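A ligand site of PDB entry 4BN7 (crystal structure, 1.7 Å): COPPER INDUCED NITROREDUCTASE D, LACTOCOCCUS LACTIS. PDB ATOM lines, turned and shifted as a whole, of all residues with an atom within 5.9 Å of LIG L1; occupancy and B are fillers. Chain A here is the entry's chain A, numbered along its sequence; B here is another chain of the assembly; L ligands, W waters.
Water W2 lies within hydrogen-bond range of O9 of LIG L1 and NH2 of Arg 10. Water W3 bridges the side-chain hydroxyl (OH) of Tyr 13 (2.9 Å) and an oxygen (O3) of LIG L1 (3.0 Å). Water W1 lies within hydrogen-bond range of N of Leu 149, OG1 of Thr 11 and N1 of LIG L1.
The backbone carbonyl oxygen (O) of Arg 10 lies within hydrogen-bond range of the indole nitrogen (NE1) of Trp 137, 3.3 Å away. A ring nitrogen (NE2) of His 151 is in hydrogen-bond range of the indole nitrogen (NE1) of Trp 124 of chain B, at 3.5 Å. The side-chain amide nitrogen (NE2) of Gln 150 is in hydrogen-bond range of the side-chain amide oxygen (OD1) of Asn 148 (2.8 Å).
An oxygen (O1) of LG2 L2 sits at hydrogen-bond distance from an oxygen (O3) of LIG L1, 2.8 Å away.
O1 of LIG L1 lies within hydrogen-bond range of OH of Tyr 13. NZ of Lys 188 lies within salt-bridge range of O7 of LIG L1 (2.7 Å). N of Thr 11 sits at hydrogen-bond distance from O9 of LIG L1 (2.8 Å). OG1 of Thr 11 is in hydrogen-bond range of O8 of LIG L1 (2.7 Å). O9 of LIG L1 is in salt-bridge range of NE of Arg 10 (2.7 Å). The guanidinium group (NH2) of Arg 9 is in salt-bridge range of an oxygen (O7) of LIG L1, at 2.8 Å. A ring nitrogen (ND1) of His 151 sits at hydrogen-bond distance from an oxygen (O2) of LIG L1 (2.9 Å). O of Leu 149 lies within hydrogen-bond range of N2 of LIG L1, at 3.0 Å. NE2 of Gln 150 sits at hydrogen-bond distance from O1 of LIG L1 (3.1 Å). The backbone NH of Phe 40 of chain B lies within hydrogen-bond range of an oxygen (O3) of LIG L1 (3.4 Å). An oxygen (O2) of LG2 L2 is in hydrogen-bond range of the backbone carbonyl oxygen of His 151, 2.7 Å away. The backbone NH (N) of Phe 40 of chain B lies within hydrogen-bond range of an oxygen (O1) of LG2 L2, at 2.7 Å.
Trp 137 touches LIG L1 (CZ2 to O8, 3.8 Å). Pro 37 of chain B touches LIG L1. O of Thr 38 of chain B touches C16 of LIG L1 (3.4 Å). Ala 39 of chain B touches LIG L1. N of Asn 41 of chain B touches O5 of LIG L1 (3.5 Å). Gln 127 of chain B touches LIG L1. Ile 131 of chain B touches LIG L1 (CD1 to C9, 3.9 Å). Hydrophobic or aromatic side chains within 4 Å of LIG L1: Tyr 13, Trp 137, Leu 149, His 151, Pro 37 of chain B, Ala 39 of chain B and Ile 131 of chain B. Of the 25 residues printed, 16 come within 4 Å of LIG L1. The nearest printed residue that does not touch LIG L1 is Trp 124 of chain B (4.02 Å).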
ATOM      1  N   ARG A   9     -28.757   5.082   6.809  1.00  0.00           N
ATOM      2  CA  ARG A   9     -28.475   3.970   5.901  1.00  0.00           C
ATOM      3  C   ARG A   9     -28.155   2.734   6.729  1.00  0.00           C
ATOM      4  O   ARG A   9     -27.276   2.765   7.590  1.00  0.00           O
ATOM      5  CB  ARG A   9     -27.308   4.300   4.953  1.00  0.00           C
ATOM      6  CG  ARG A   9     -26.940   3.185   3.979  1.00  0.00           C
ATOM      7  CD  ARG A   9     -25.444   3.012   3.825  1.00  0.00           C
ATOM      8  NE  ARG A   9     -24.821   2.850   5.129  1.00  0.00           N
ATOM      9  CZ  ARG A   9     -24.790   1.712   5.821  1.00  0.00           C
ATOM     10  NH1 ARG A   9     -25.327   0.594   5.333  1.00  0.00           N
ATOM     11  NH2 ARG A   9     -24.224   1.686   7.014  1.00  0.00           N
ATOM     12  N   ARG A  10     -28.858   1.651   6.466  1.00  0.00           N
ATOM     13  CA  ARG A  10     -28.630   0.398   7.174  1.00  0.00           C
ATOM     14  C   ARG A  10     -28.836  -0.777   6.235  1.00  0.00           C
ATOM     15  O   ARG A  10     -29.476  -0.648   5.191  1.00  0.00           O
ATOM     16  CB  ARG A  10     -29.555   0.265   8.371  1.00  0.00           C
ATOM     17  CG  ARG A  10     -29.328   1.269   9.488  1.00  0.00           C
ATOM     18  CD  ARG A  10     -27.975   1.113  10.180  1.00  0.00           C
ATOM     19  NE  ARG A  10     -27.752  -0.241  10.678  1.00  0.00           N
ATOM     20  CZ  ARG A  10     -28.297  -0.736  11.784  1.00  0.00           C
ATOM     21  NH1 ARG A  10     -29.081  -0.003  12.550  1.00  0.00           N
ATOM     22  NH2 ARG A  10     -28.039  -1.990  12.128  1.00  0.00           N
ATOM     23  N   THR A  11     -28.272  -1.921   6.617  1.00  0.00           N
ATOM     24  CA  THR A  11     -28.541  -3.170   5.920  1.00  0.00           C
ATOM     25  C   THR A  11     -29.932  -3.663   6.280  1.00  0.00           C
ATOM     26  O   THR A  11     -30.235  -3.931   7.452  1.00  0.00           O
ATOM     27  CB  THR A  11     -27.516  -4.241   6.310  1.00  0.00           C
ATOM     28  OG1 THR A  11     -26.242  -3.909   5.747  1.00  0.00           O
ATOM     29  CG2 THR A  11     -27.947  -5.620   5.811  1.00  0.00           C
ATOM     30  N   ILE A  12     -30.784  -3.780   5.258  1.00  0.00           N
ATOM     31  CA  ILE A  12     -32.149  -4.236   5.409  1.00  0.00           C
ATOM     32  C   ILE A  12     -32.307  -5.485   4.556  1.00  0.00           C
ATOM     33  O   ILE A  12     -32.220  -5.421   3.325  1.00  0.00           O
ATOM     34  CB  ILE A  12     -33.148  -3.162   4.928  1.00  0.00           C
ATOM     35  CG1 ILE A  12     -32.966  -1.852   5.694  1.00  0.00           C
ATOM     36  CG2 ILE A  12     -34.586  -3.668   5.054  1.00  0.00           C
ATOM     37  CD1 ILE A  12     -33.257  -1.967   7.190  1.00  0.00           C
ATOM     38  N   TYR A  13     -32.533  -6.616   5.196  1.00  0.00           N
ATOM     39  CA  TYR A  13     -32.696  -7.872   4.459  1.00  0.00           C
ATOM     40  C   TYR A  13     -34.139  -8.139   4.053  1.00  0.00           C
ATOM     41  O   TYR A  13     -34.385  -8.802   3.051  1.00  0.00           O
ATOM     42  CB  TYR A  13     -32.134  -9.043   5.271  1.00  0.00           C
ATOM     43  CG  TYR A  13     -30.632  -9.033   5.385  1.00  0.00           C
ATOM     44  CD1 TYR A  13     -29.823  -9.190   4.269  1.00  0.00           C
ATOM     45  CD2 TYR A  13     -30.017  -8.860   6.620  1.00  0.00           C
ATOM     46  CE1 TYR A  13     -28.443  -9.186   4.377  1.00  0.00           C
ATOM     47  CE2 TYR A  13     -28.645  -8.855   6.743  1.00  0.00           C
ATOM     48  CZ  TYR A  13     -27.864  -9.008   5.618  1.00  0.00           C
ATOM     49  OH  TYR A  13     -26.493  -9.009   5.754  1.00  0.00           O
ATOM     50  N   PHE A  91     -33.841 -12.157  -1.478  1.00  0.00           N
ATOM     51  CA  PHE A  91     -33.268 -11.236  -2.446  1.00  0.00           C
ATOM     52  C   PHE A  91     -34.222 -11.048  -3.633  1.00  0.00           C
ATOM     53  O   PHE A  91     -34.486  -9.920  -4.050  1.00  0.00           O
ATOM     54  CB  PHE A  91     -31.897 -11.729  -2.916  1.00  0.00           C
ATOM     55  CG  PHE A  91     -30.883 -11.867  -1.810  1.00  0.00           C
ATOM     56  CD1 PHE A  91     -30.785 -10.899  -0.827  1.00  0.00           C
ATOM     57  CD2 PHE A  91     -30.041 -12.965  -1.753  1.00  0.00           C
ATOM     58  CE1 PHE A  91     -29.861 -11.024   0.199  1.00  0.00           C
ATOM     59  CE2 PHE A  91     -29.105 -13.088  -0.734  1.00  0.00           C
ATOM     60  CZ  PHE A  91     -29.024 -12.122   0.247  1.00  0.00           C
ATOM     61  N   VAL A 134     -21.841   2.835  -1.619  1.00  0.00           N
ATOM     62  CA  VAL A 134     -22.426   3.377  -0.390  1.00  0.00           C
ATOM     63  C   VAL A 134     -23.157   4.699  -0.641  1.00  0.00           C
ATOM     64  O   VAL A 134     -24.154   4.978   0.026  1.00  0.00           O
ATOM     65  CB  VAL A 134     -21.410   3.541   0.758  1.00  0.00           C
ATOM     66  CG1 VAL A 134     -20.748   2.201   1.057  1.00  0.00           C
ATOM     67  CG2 VAL A 134     -20.394   4.628   0.448  1.00  0.00           C
ATOM     68  N   TRP A 137     -26.466   3.517  -1.907  1.00  0.00           N
ATOM     69  CA  TRP A 137     -27.118   2.880  -0.764  1.00  0.00           C
ATOM     70  C   TRP A 137     -27.738   3.943   0.129  1.00  0.00           C
ATOM     71  O   TRP A 137     -28.897   3.860   0.527  1.00  0.00           O
ATOM     72  CB  TRP A 137     -26.065   2.080  -0.004  1.00  0.00           C
ATOM     73  CG  TRP A 137     -26.539   1.034   0.974  1.00  0.00           C
ATOM     74  CD1 TRP A 137     -27.796   0.849   1.478  1.00  0.00           C
ATOM     75  CD2 TRP A 137     -25.718   0.021   1.549  1.00  0.00           C
ATOM     76  NE1 TRP A 137     -27.803  -0.231   2.339  1.00  0.00           N
ATOM     77  CE2 TRP A 137     -26.534  -0.760   2.397  1.00  0.00           C
ATOM     78  CE3 TRP A 137     -24.368  -0.306   1.430  1.00  0.00           C
ATOM     79  CZ2 TRP A 137     -26.040  -1.830   3.119  1.00  0.00           C
ATOM     80  CZ3 TRP A 137     -23.880  -1.363   2.143  1.00  0.00           C
ATOM     81  CH2 TRP A 137     -24.714  -2.126   2.975  1.00  0.00           C
ATOM     82  N   ASN A 148     -29.450  -4.074   0.760  1.00  0.00           N
ATOM     83  CA  ASN A 148     -28.356  -4.849   1.305  1.00  0.00           C
ATOM     84  C   ASN A 148     -27.387  -5.163   0.172  1.00  0.00           C
ATOM     85  O   ASN A 148     -27.776  -5.189  -0.990  1.00  0.00           O
ATOM     86  CB  ASN A 148     -28.862  -6.108   2.021  1.00  0.00           C
ATOM     87  CG  ASN A 148     -29.603  -7.063   1.087  1.00  0.00           C
ATOM     88  OD1 ASN A 148     -28.991  -7.845   0.368  1.00  0.00           O
ATOM     89  ND2 ASN A 148     -30.928  -7.030   1.138  1.00  0.00           N
ATOM     90  N   LEU A 149     -26.116  -5.358   0.527  1.00  0.00           N
ATOM     91  CA  LEU A 149     -25.048  -5.495  -0.452  1.00  0.00           C
ATOM     92  C   LEU A 149     -24.536  -6.927  -0.460  1.00  0.00           C
ATOM     93  O   LEU A 149     -24.102  -7.439   0.587  1.00  0.00           O
ATOM     94  CB  LEU A 149     -23.908  -4.522  -0.124  1.00  0.00           C
ATOM     95  CG  LEU A 149     -22.708  -4.502  -1.074  1.00  0.00           C
ATOM     96  CD1 LEU A 149     -23.155  -4.021  -2.447  1.00  0.00           C
ATOM     97  CD2 LEU A 149     -21.586  -3.622  -0.525  1.00  0.00           C
ATOM     98  N   GLN A 150     -24.584  -7.575  -1.618  1.00  0.00           N
ATOM     99  CA  GLN A 150     -24.191  -8.972  -1.762  1.00  0.00           C
ATOM    100  C   GLN A 150     -22.995  -9.114  -2.692  1.00  0.00           C
ATOM    101  O   GLN A 150     -22.686  -8.191  -3.461  1.00  0.00           O
ATOM    102  CB  GLN A 150     -25.357  -9.798  -2.297  1.00  0.00           C
ATOM    103  CG  GLN A 150     -26.574  -9.816  -1.395  1.00  0.00           C
ATOM    104  CD  GLN A 150     -26.228 -10.182   0.027  1.00  0.00           C
ATOM    105  OE1 GLN A 150     -25.432 -11.100   0.266  1.00  0.00           O
ATOM    106  NE2 GLN A 150     -26.792  -9.464   0.989  1.00  0.00           N
ATOM    107  N   HIS A 151     -22.347 -10.266  -2.632  1.00  0.00           N
ATOM    108  CA  HIS A 151     -21.180 -10.539  -3.464  1.00  0.00           C
ATOM    109  C   HIS A 151     -21.180 -11.947  -4.040  1.00  0.00           C
ATOM    110  O   HIS A 151     -20.487 -12.844  -3.562  1.00  0.00           O
ATOM    111  CB  HIS A 151     -19.899 -10.269  -2.675  1.00  0.00           C
ATOM    112  CG  HIS A 151     -19.742  -8.839  -2.303  1.00  0.00           C
ATOM    113  ND1 HIS A 151     -20.252  -8.315  -1.132  1.00  0.00           N
ATOM    114  CD2 HIS A 151     -19.180  -7.799  -2.965  1.00  0.00           C
ATOM    115  CE1 HIS A 151     -19.993  -7.026  -1.077  1.00  0.00           C
ATOM    116  NE2 HIS A 151     -19.350  -6.685  -2.180  1.00  0.00           N
ATOM    117  N   ALA A 185     -33.817  -2.835  10.619  1.00  0.00           N
ATOM    118  CA  ALA A 185     -32.451  -3.334  10.670  1.00  0.00           C
ATOM    119  C   ALA A 185     -32.202  -3.948  12.045  1.00  0.00           C
ATOM    120  O   ALA A 185     -32.896  -3.626  13.017  1.00  0.00           O
ATOM    121  CB  ALA A 185     -31.482  -2.213  10.413  1.00  0.00           C
ATOM    122  N   LYS A 188     -26.576  -3.107  15.947  1.00  0.00           N
ATOM    123  CA  LYS A 188     -25.215  -2.945  15.473  1.00  0.00           C
ATOM    124  C   LYS A 188     -24.368  -2.318  16.560  1.00  0.00           C
ATOM    125  O   LYS A 188     -24.807  -1.421  17.259  1.00  0.00           O
ATOM    126  CB  LYS A 188     -25.149  -2.051  14.221  1.00  0.00           C
ATOM    127  CG  LYS A 188     -23.736  -1.903  13.689  1.00  0.00           C
ATOM    128  CD  LYS A 188     -23.684  -1.237  12.337  1.00  0.00           C
ATOM    129  CE  LYS A 188     -24.180   0.187  12.406  1.00  0.00           C
ATOM    130  NZ  LYS A 188     -23.967   0.878  11.106  1.00  0.00           N
ATOM    131  N   PHE B  35     -20.411   5.926  11.207  1.00  0.00           N
ATOM    132  CA  PHE B  35     -21.631   5.520  10.538  1.00  0.00           C
ATOM    133  C   PHE B  35     -21.423   4.992   9.114  1.00  0.00           C
ATOM    134  O   PHE B  35     -22.377   4.791   8.366  1.00  0.00           O
ATOM    135  CB  PHE B  35     -22.645   6.665  10.584  1.00  0.00           C
ATOM    136  CG  PHE B  35     -23.063   7.037  11.996  1.00  0.00           C
ATOM    137  CD1 PHE B  35     -23.529   6.057  12.873  1.00  0.00           C
ATOM    138  CD2 PHE B  35     -22.945   8.333  12.448  1.00  0.00           C
ATOM    139  CE1 PHE B  35     -23.894   6.383  14.164  1.00  0.00           C
ATOM    140  CE2 PHE B  35     -23.325   8.672  13.744  1.00  0.00           C
ATOM    141  CZ  PHE B  35     -23.794   7.691  14.611  1.00  0.00           C
ATOM    142  N   SER B  36     -20.169   4.718   8.767  1.00  0.00           N
ATOM    143  CA  SER B  36     -19.843   4.111   7.473  1.00  0.00           C
ATOM    144  C   SER B  36     -19.895   2.588   7.566  1.00  0.00           C
ATOM    145  O   SER B  36     -19.394   1.999   8.531  1.00  0.00           O
ATOM    146  CB  SER B  36     -18.429   4.514   7.022  1.00  0.00           C
ATOM    147  OG  SER B  36     -18.316   5.896   6.769  1.00  0.00           O
ATOM    148  N   PRO B  37     -20.488   1.935   6.568  1.00  0.00           N
ATOM    149  CA  PRO B  37     -20.508   0.468   6.604  1.00  0.00           C
ATOM    150  C   PRO B  37     -19.168  -0.184   6.225  1.00  0.00           C
ATOM    151  O   PRO B  37     -18.406   0.381   5.430  1.00  0.00           O
ATOM    152  CB  PRO B  37     -21.555   0.124   5.561  1.00  0.00           C
ATOM    153  CG  PRO B  37     -21.429   1.206   4.561  1.00  0.00           C
ATOM    154  CD  PRO B  37     -21.134   2.457   5.356  1.00  0.00           C
ATOM    155  N   THR B  38     -18.904  -1.358   6.794  1.00  0.00           N
ATOM    156  CA  THR B  38     -17.742  -2.174   6.467  1.00  0.00           C
ATOM    157  C   THR B  38     -18.131  -3.650   6.464  1.00  0.00           C
ATOM    158  O   THR B  38     -19.053  -4.060   7.164  1.00  0.00           O
ATOM    159  CB  THR B  38     -16.607  -1.995   7.475  1.00  0.00           C
ATOM    160  OG1 THR B  38     -17.111  -2.149   8.812  1.00  0.00           O
ATOM    161  CG2 THR B  38     -15.967  -0.627   7.320  1.00  0.00           C
ATOM    162  N   ALA B  39     -17.434  -4.444   5.659  1.00  0.00           N
ATOM    163  CA  ALA B  39     -17.729  -5.866   5.580  1.00  0.00           C
ATOM    164  C   ALA B  39     -17.703  -6.493   6.967  1.00  0.00           C
ATOM    165  O   ALA B  39     -16.748  -6.327   7.729  1.00  0.00           O
ATOM    166  CB  ALA B  39     -16.741  -6.548   4.661  1.00  0.00           C
ATOM    167  N   PHE B  40     -18.796  -7.156   7.333  1.00  0.00           N
ATOM    168  CA  PHE B  40     -18.881  -7.918   8.578  1.00  0.00           C
ATOM    169  C   PHE B  40     -18.834  -6.989   9.783  1.00  0.00           C
ATOM    170  O   PHE B  40     -18.536  -7.430  10.900  1.00  0.00           O
ATOM    171  CB  PHE B  40     -17.749  -8.941   8.684  1.00  0.00           C
ATOM    172  CG  PHE B  40     -18.034 -10.249   7.980  1.00  0.00           C
ATOM    173  CD1 PHE B  40     -17.849 -10.370   6.609  1.00  0.00           C
ATOM    174  CD2 PHE B  40     -18.470 -11.345   8.698  1.00  0.00           C
ATOM    175  CE1 PHE B  40     -18.108 -11.572   5.970  1.00  0.00           C
ATOM    176  CE2 PHE B  40     -18.734 -12.554   8.062  1.00  0.00           C
ATOM    177  CZ  PHE B  40     -18.546 -12.660   6.699  1.00  0.00           C
ATOM    178  N   ASN B  41     -19.134  -5.717   9.547  1.00  0.00           N
ATOM    179  CA  ASN B  41     -18.985  -4.683  10.576  1.00  0.00           C
ATOM    180  C   ASN B  41     -17.572  -4.720  11.167  1.00  0.00           C
ATOM    181  O   ASN B  41     -17.389  -4.499  12.353  1.00  0.00           O
ATOM    182  CB  ASN B  41     -20.032  -4.857  11.670  1.00  0.00           C
ATOM    183  CG  ASN B  41     -20.169  -3.627  12.549  1.00  0.00           C
ATOM    184  OD1 ASN B  41     -20.016  -2.497  12.092  1.00  0.00           O
ATOM    185  ND2 ASN B  41     -20.449  -3.847  13.850  1.00  0.00           N
ATOM    186  N   TRP B 124     -12.440  -5.885   0.287  1.00  0.00           N
ATOM    187  CA  TRP B 124     -13.477  -5.170   1.036  1.00  0.00           C
ATOM    188  C   TRP B 124     -12.868  -4.102   1.943  1.00  0.00           C
ATOM    189  O   TRP B 124     -13.489  -3.055   2.175  1.00  0.00           O
ATOM    190  CB  TRP B 124     -14.314  -6.155   1.851  1.00  0.00           C
ATOM    191  CG  TRP B 124     -15.190  -7.040   0.988  1.00  0.00           C
ATOM    192  CD1 TRP B 124     -15.645  -6.766  -0.267  1.00  0.00           C
ATOM    193  CD2 TRP B 124     -15.682  -8.339   1.319  1.00  0.00           C
ATOM    194  NE1 TRP B 124     -16.401  -7.818  -0.743  1.00  0.00           N
ATOM    195  CE2 TRP B 124     -16.445  -8.795   0.214  1.00  0.00           C
ATOM    196  CE3 TRP B 124     -15.572  -9.161   2.441  1.00  0.00           C
ATOM    197  CZ2 TRP B 124     -17.071 -10.023   0.211  1.00  0.00           C
ATOM    198  CZ3 TRP B 124     -16.197 -10.383   2.425  1.00  0.00           C
ATOM    199  CH2 TRP B 124     -16.941 -10.809   1.329  1.00  0.00           C
ATOM    200  N   GLN B 127     -12.149  -1.144  -0.327  1.00  0.00           N
ATOM    201  CA  GLN B 127     -13.416  -0.455  -0.551  1.00  0.00           C
ATOM    202  C   GLN B 127     -13.792   0.379   0.686  1.00  0.00           C
ATOM    203  O   GLN B 127     -14.210   1.535   0.579  1.00  0.00           O
ATOM    204  CB  GLN B 127     -14.508  -1.462  -0.931  1.00  0.00           C
ATOM    205  CG  GLN B 127     -14.251  -2.116  -2.287  1.00  0.00           C
ATOM    206  CD  GLN B 127     -15.196  -3.241  -2.626  1.00  0.00           C
ATOM    207  OE1 GLN B 127     -16.050  -3.609  -1.819  1.00  0.00           O
ATOM    208  NE2 GLN B 127     -15.043  -3.801  -3.817  1.00  0.00           N
ATOM    209  N   GLY B 128     -13.616  -0.219   1.871  1.00  0.00           N
ATOM    210  CA  GLY B 128     -13.897   0.468   3.122  1.00  0.00           C
ATOM    211  C   GLY B 128     -13.090   1.740   3.300  1.00  0.00           C
ATOM    212  O   GLY B 128     -13.571   2.723   3.862  1.00  0.00           O
ATOM    213  N   ILE B 131     -14.680   4.310   1.206  1.00  0.00           N
ATOM    214  CA  ILE B 131     -15.948   4.667   1.831  1.00  0.00           C
ATOM    215  C   ILE B 131     -15.771   5.695   2.947  1.00  0.00           C
ATOM    216  O   ILE B 131     -16.424   6.751   2.959  1.00  0.00           O
ATOM    217  CB  ILE B 131     -16.671   3.395   2.353  1.00  0.00           C
ATOM    218  CG1 ILE B 131     -17.209   2.564   1.191  1.00  0.00           C
ATOM    219  CG2 ILE B 131     -17.808   3.772   3.304  1.00  0.00           C
ATOM    220  CD1 ILE B 131     -17.528   1.112   1.533  1.00  0.00           C
HETATM  221  N1  LIG L   1     -23.626  -7.804   3.786  1.00  0.00           N
HETATM  222  C1  LIG L   1     -24.138  -9.109   3.229  1.00  0.00           C
HETATM  223  O1  LIG L   1     -25.200  -9.513   3.594  1.00  0.00           O
HETATM  224  N2  LIG L   1     -23.330  -9.817   2.280  1.00  0.00           N
HETATM  225  C2  LIG L   1     -22.106  -9.344   1.871  1.00  0.00           C
HETATM  226  O2  LIG L   1     -21.498  -9.894   1.014  1.00  0.00           O
HETATM  227  C3  LIG L   1     -21.609  -8.077   2.406  1.00  0.00           C
HETATM  228  N3  LIG L   1     -20.470  -7.614   2.063  1.00  0.00           N
HETATM  229  C4  LIG L   1     -20.144  -6.173   2.361  1.00  0.00           C
HETATM  230  C5  LIG L   1     -18.963  -5.510   1.670  1.00  0.00           C
HETATM  231  C6  LIG L   1     -18.689  -4.241   1.923  1.00  0.00           C
HETATM  232  C7  LIG L   1     -17.492  -3.546   1.266  1.00  0.00           C
HETATM  233  C8  LIG L   1     -19.558  -3.445   2.904  1.00  0.00           C
HETATM  234  C9  LIG L   1     -19.269  -1.976   3.148  1.00  0.00           C
HETATM  235  C10 LIG L   1     -20.578  -4.027   3.516  1.00  0.00           C
HETATM  236  C11 LIG L   1     -20.899  -5.486   3.241  1.00  0.00           C
HETATM  237  N4  LIG L   1     -22.009  -6.123   3.904  1.00  0.00           N
HETATM  238  C12 LIG L   1     -22.451  -7.333   3.403  1.00  0.00           C
HETATM  239  C13 LIG L   1     -22.846  -5.398   4.844  1.00  0.00           C
HETATM  240  C14 LIG L   1     -22.096  -5.156   6.150  1.00  0.00           C
HETATM  241  O3  LIG L   1     -22.070  -6.340   6.906  1.00  0.00           O
HETATM  242  C15 LIG L   1     -22.825  -4.048   6.911  1.00  0.00           C
HETATM  243  O4  LIG L   1     -22.679  -2.876   6.150  1.00  0.00           O
HETATM  244  C16 LIG L   1     -22.233  -3.893   8.317  1.00  0.00           C
HETATM  245  O5  LIG L   1     -22.539  -5.028   9.098  1.00  0.00           O
HETATM  246  C17 LIG L   1     -22.820  -2.674   9.029  1.00  0.00           C
HETATM  247  O6  LIG L   1     -24.201  -2.816   9.106  1.00  0.00           O
HETATM  248  P1  LIG L   1     -25.148  -1.659   8.409  1.00  0.00           P
HETATM  249  O7  LIG L   1     -24.667  -0.337   8.844  1.00  0.00           O
HETATM  250  O8  LIG L   1     -24.984  -1.792   6.791  1.00  0.00           O
HETATM  251  O9  LIG L   1     -26.668  -1.986   8.880  1.00  0.00           O
HETATM  252  C1  LG2 L   2     -22.188 -11.657   5.051  1.00  0.00           C
HETATM  253  C2  LG2 L   2     -21.958 -10.413   5.621  1.00  0.00           C
HETATM  254 CL1  LG2 L   2     -22.994  -9.772   6.850  1.00  0.00          CL
HETATM  255  C3  LG2 L   2     -20.885  -9.656   5.198  1.00  0.00           C
HETATM  256  O1  LG2 L   2     -20.661  -8.440   5.786  1.00  0.00           O
HETATM  257  C4  LG2 L   2     -20.009 -10.109   4.240  1.00  0.00           C
HETATM  258 CL2  LG2 L   2     -18.685  -9.081   3.795  1.00  0.00          CL
HETATM  259  C5  LG2 L   2     -20.221 -11.345   3.660  1.00  0.00           C
HETATM  260  C6  LG2 L   2     -21.313 -12.113   4.060  1.00  0.00           C
HETATM  261  N1  LG2 L   2     -21.537 -13.413   3.493  1.00  0.00           N
HETATM  262  C7  LG2 L   2     -21.675 -13.631   2.082  1.00  0.00           C
HETATM  263  C8  LG2 L   2     -22.894 -14.061   1.584  1.00  0.00           C
HETATM  264  C9  LG2 L   2     -23.044 -14.298   0.225  1.00  0.00           C
HETATM  265  C10 LG2 L   2     -21.971 -14.105  -0.626  1.00  0.00           C
HETATM  266  O2  LG2 L   2     -22.116 -14.342  -1.975  1.00  0.00           O
HETATM  267  C11 LG2 L   2     -20.745 -13.682  -0.130  1.00  0.00           C
HETATM  268  C12 LG2 L   2     -20.601 -13.452   1.232  1.00  0.00           C
HETATM  269  O   HOH W   1     -25.734  -5.534   3.391  1.00  0.00           O
HETATM  270  O   HOH W   2     -26.811  -3.861  10.567  1.00  0.00           O
HETATM  271  O   HOH W   3     -24.852  -7.312   7.409  1.00  0.00           O
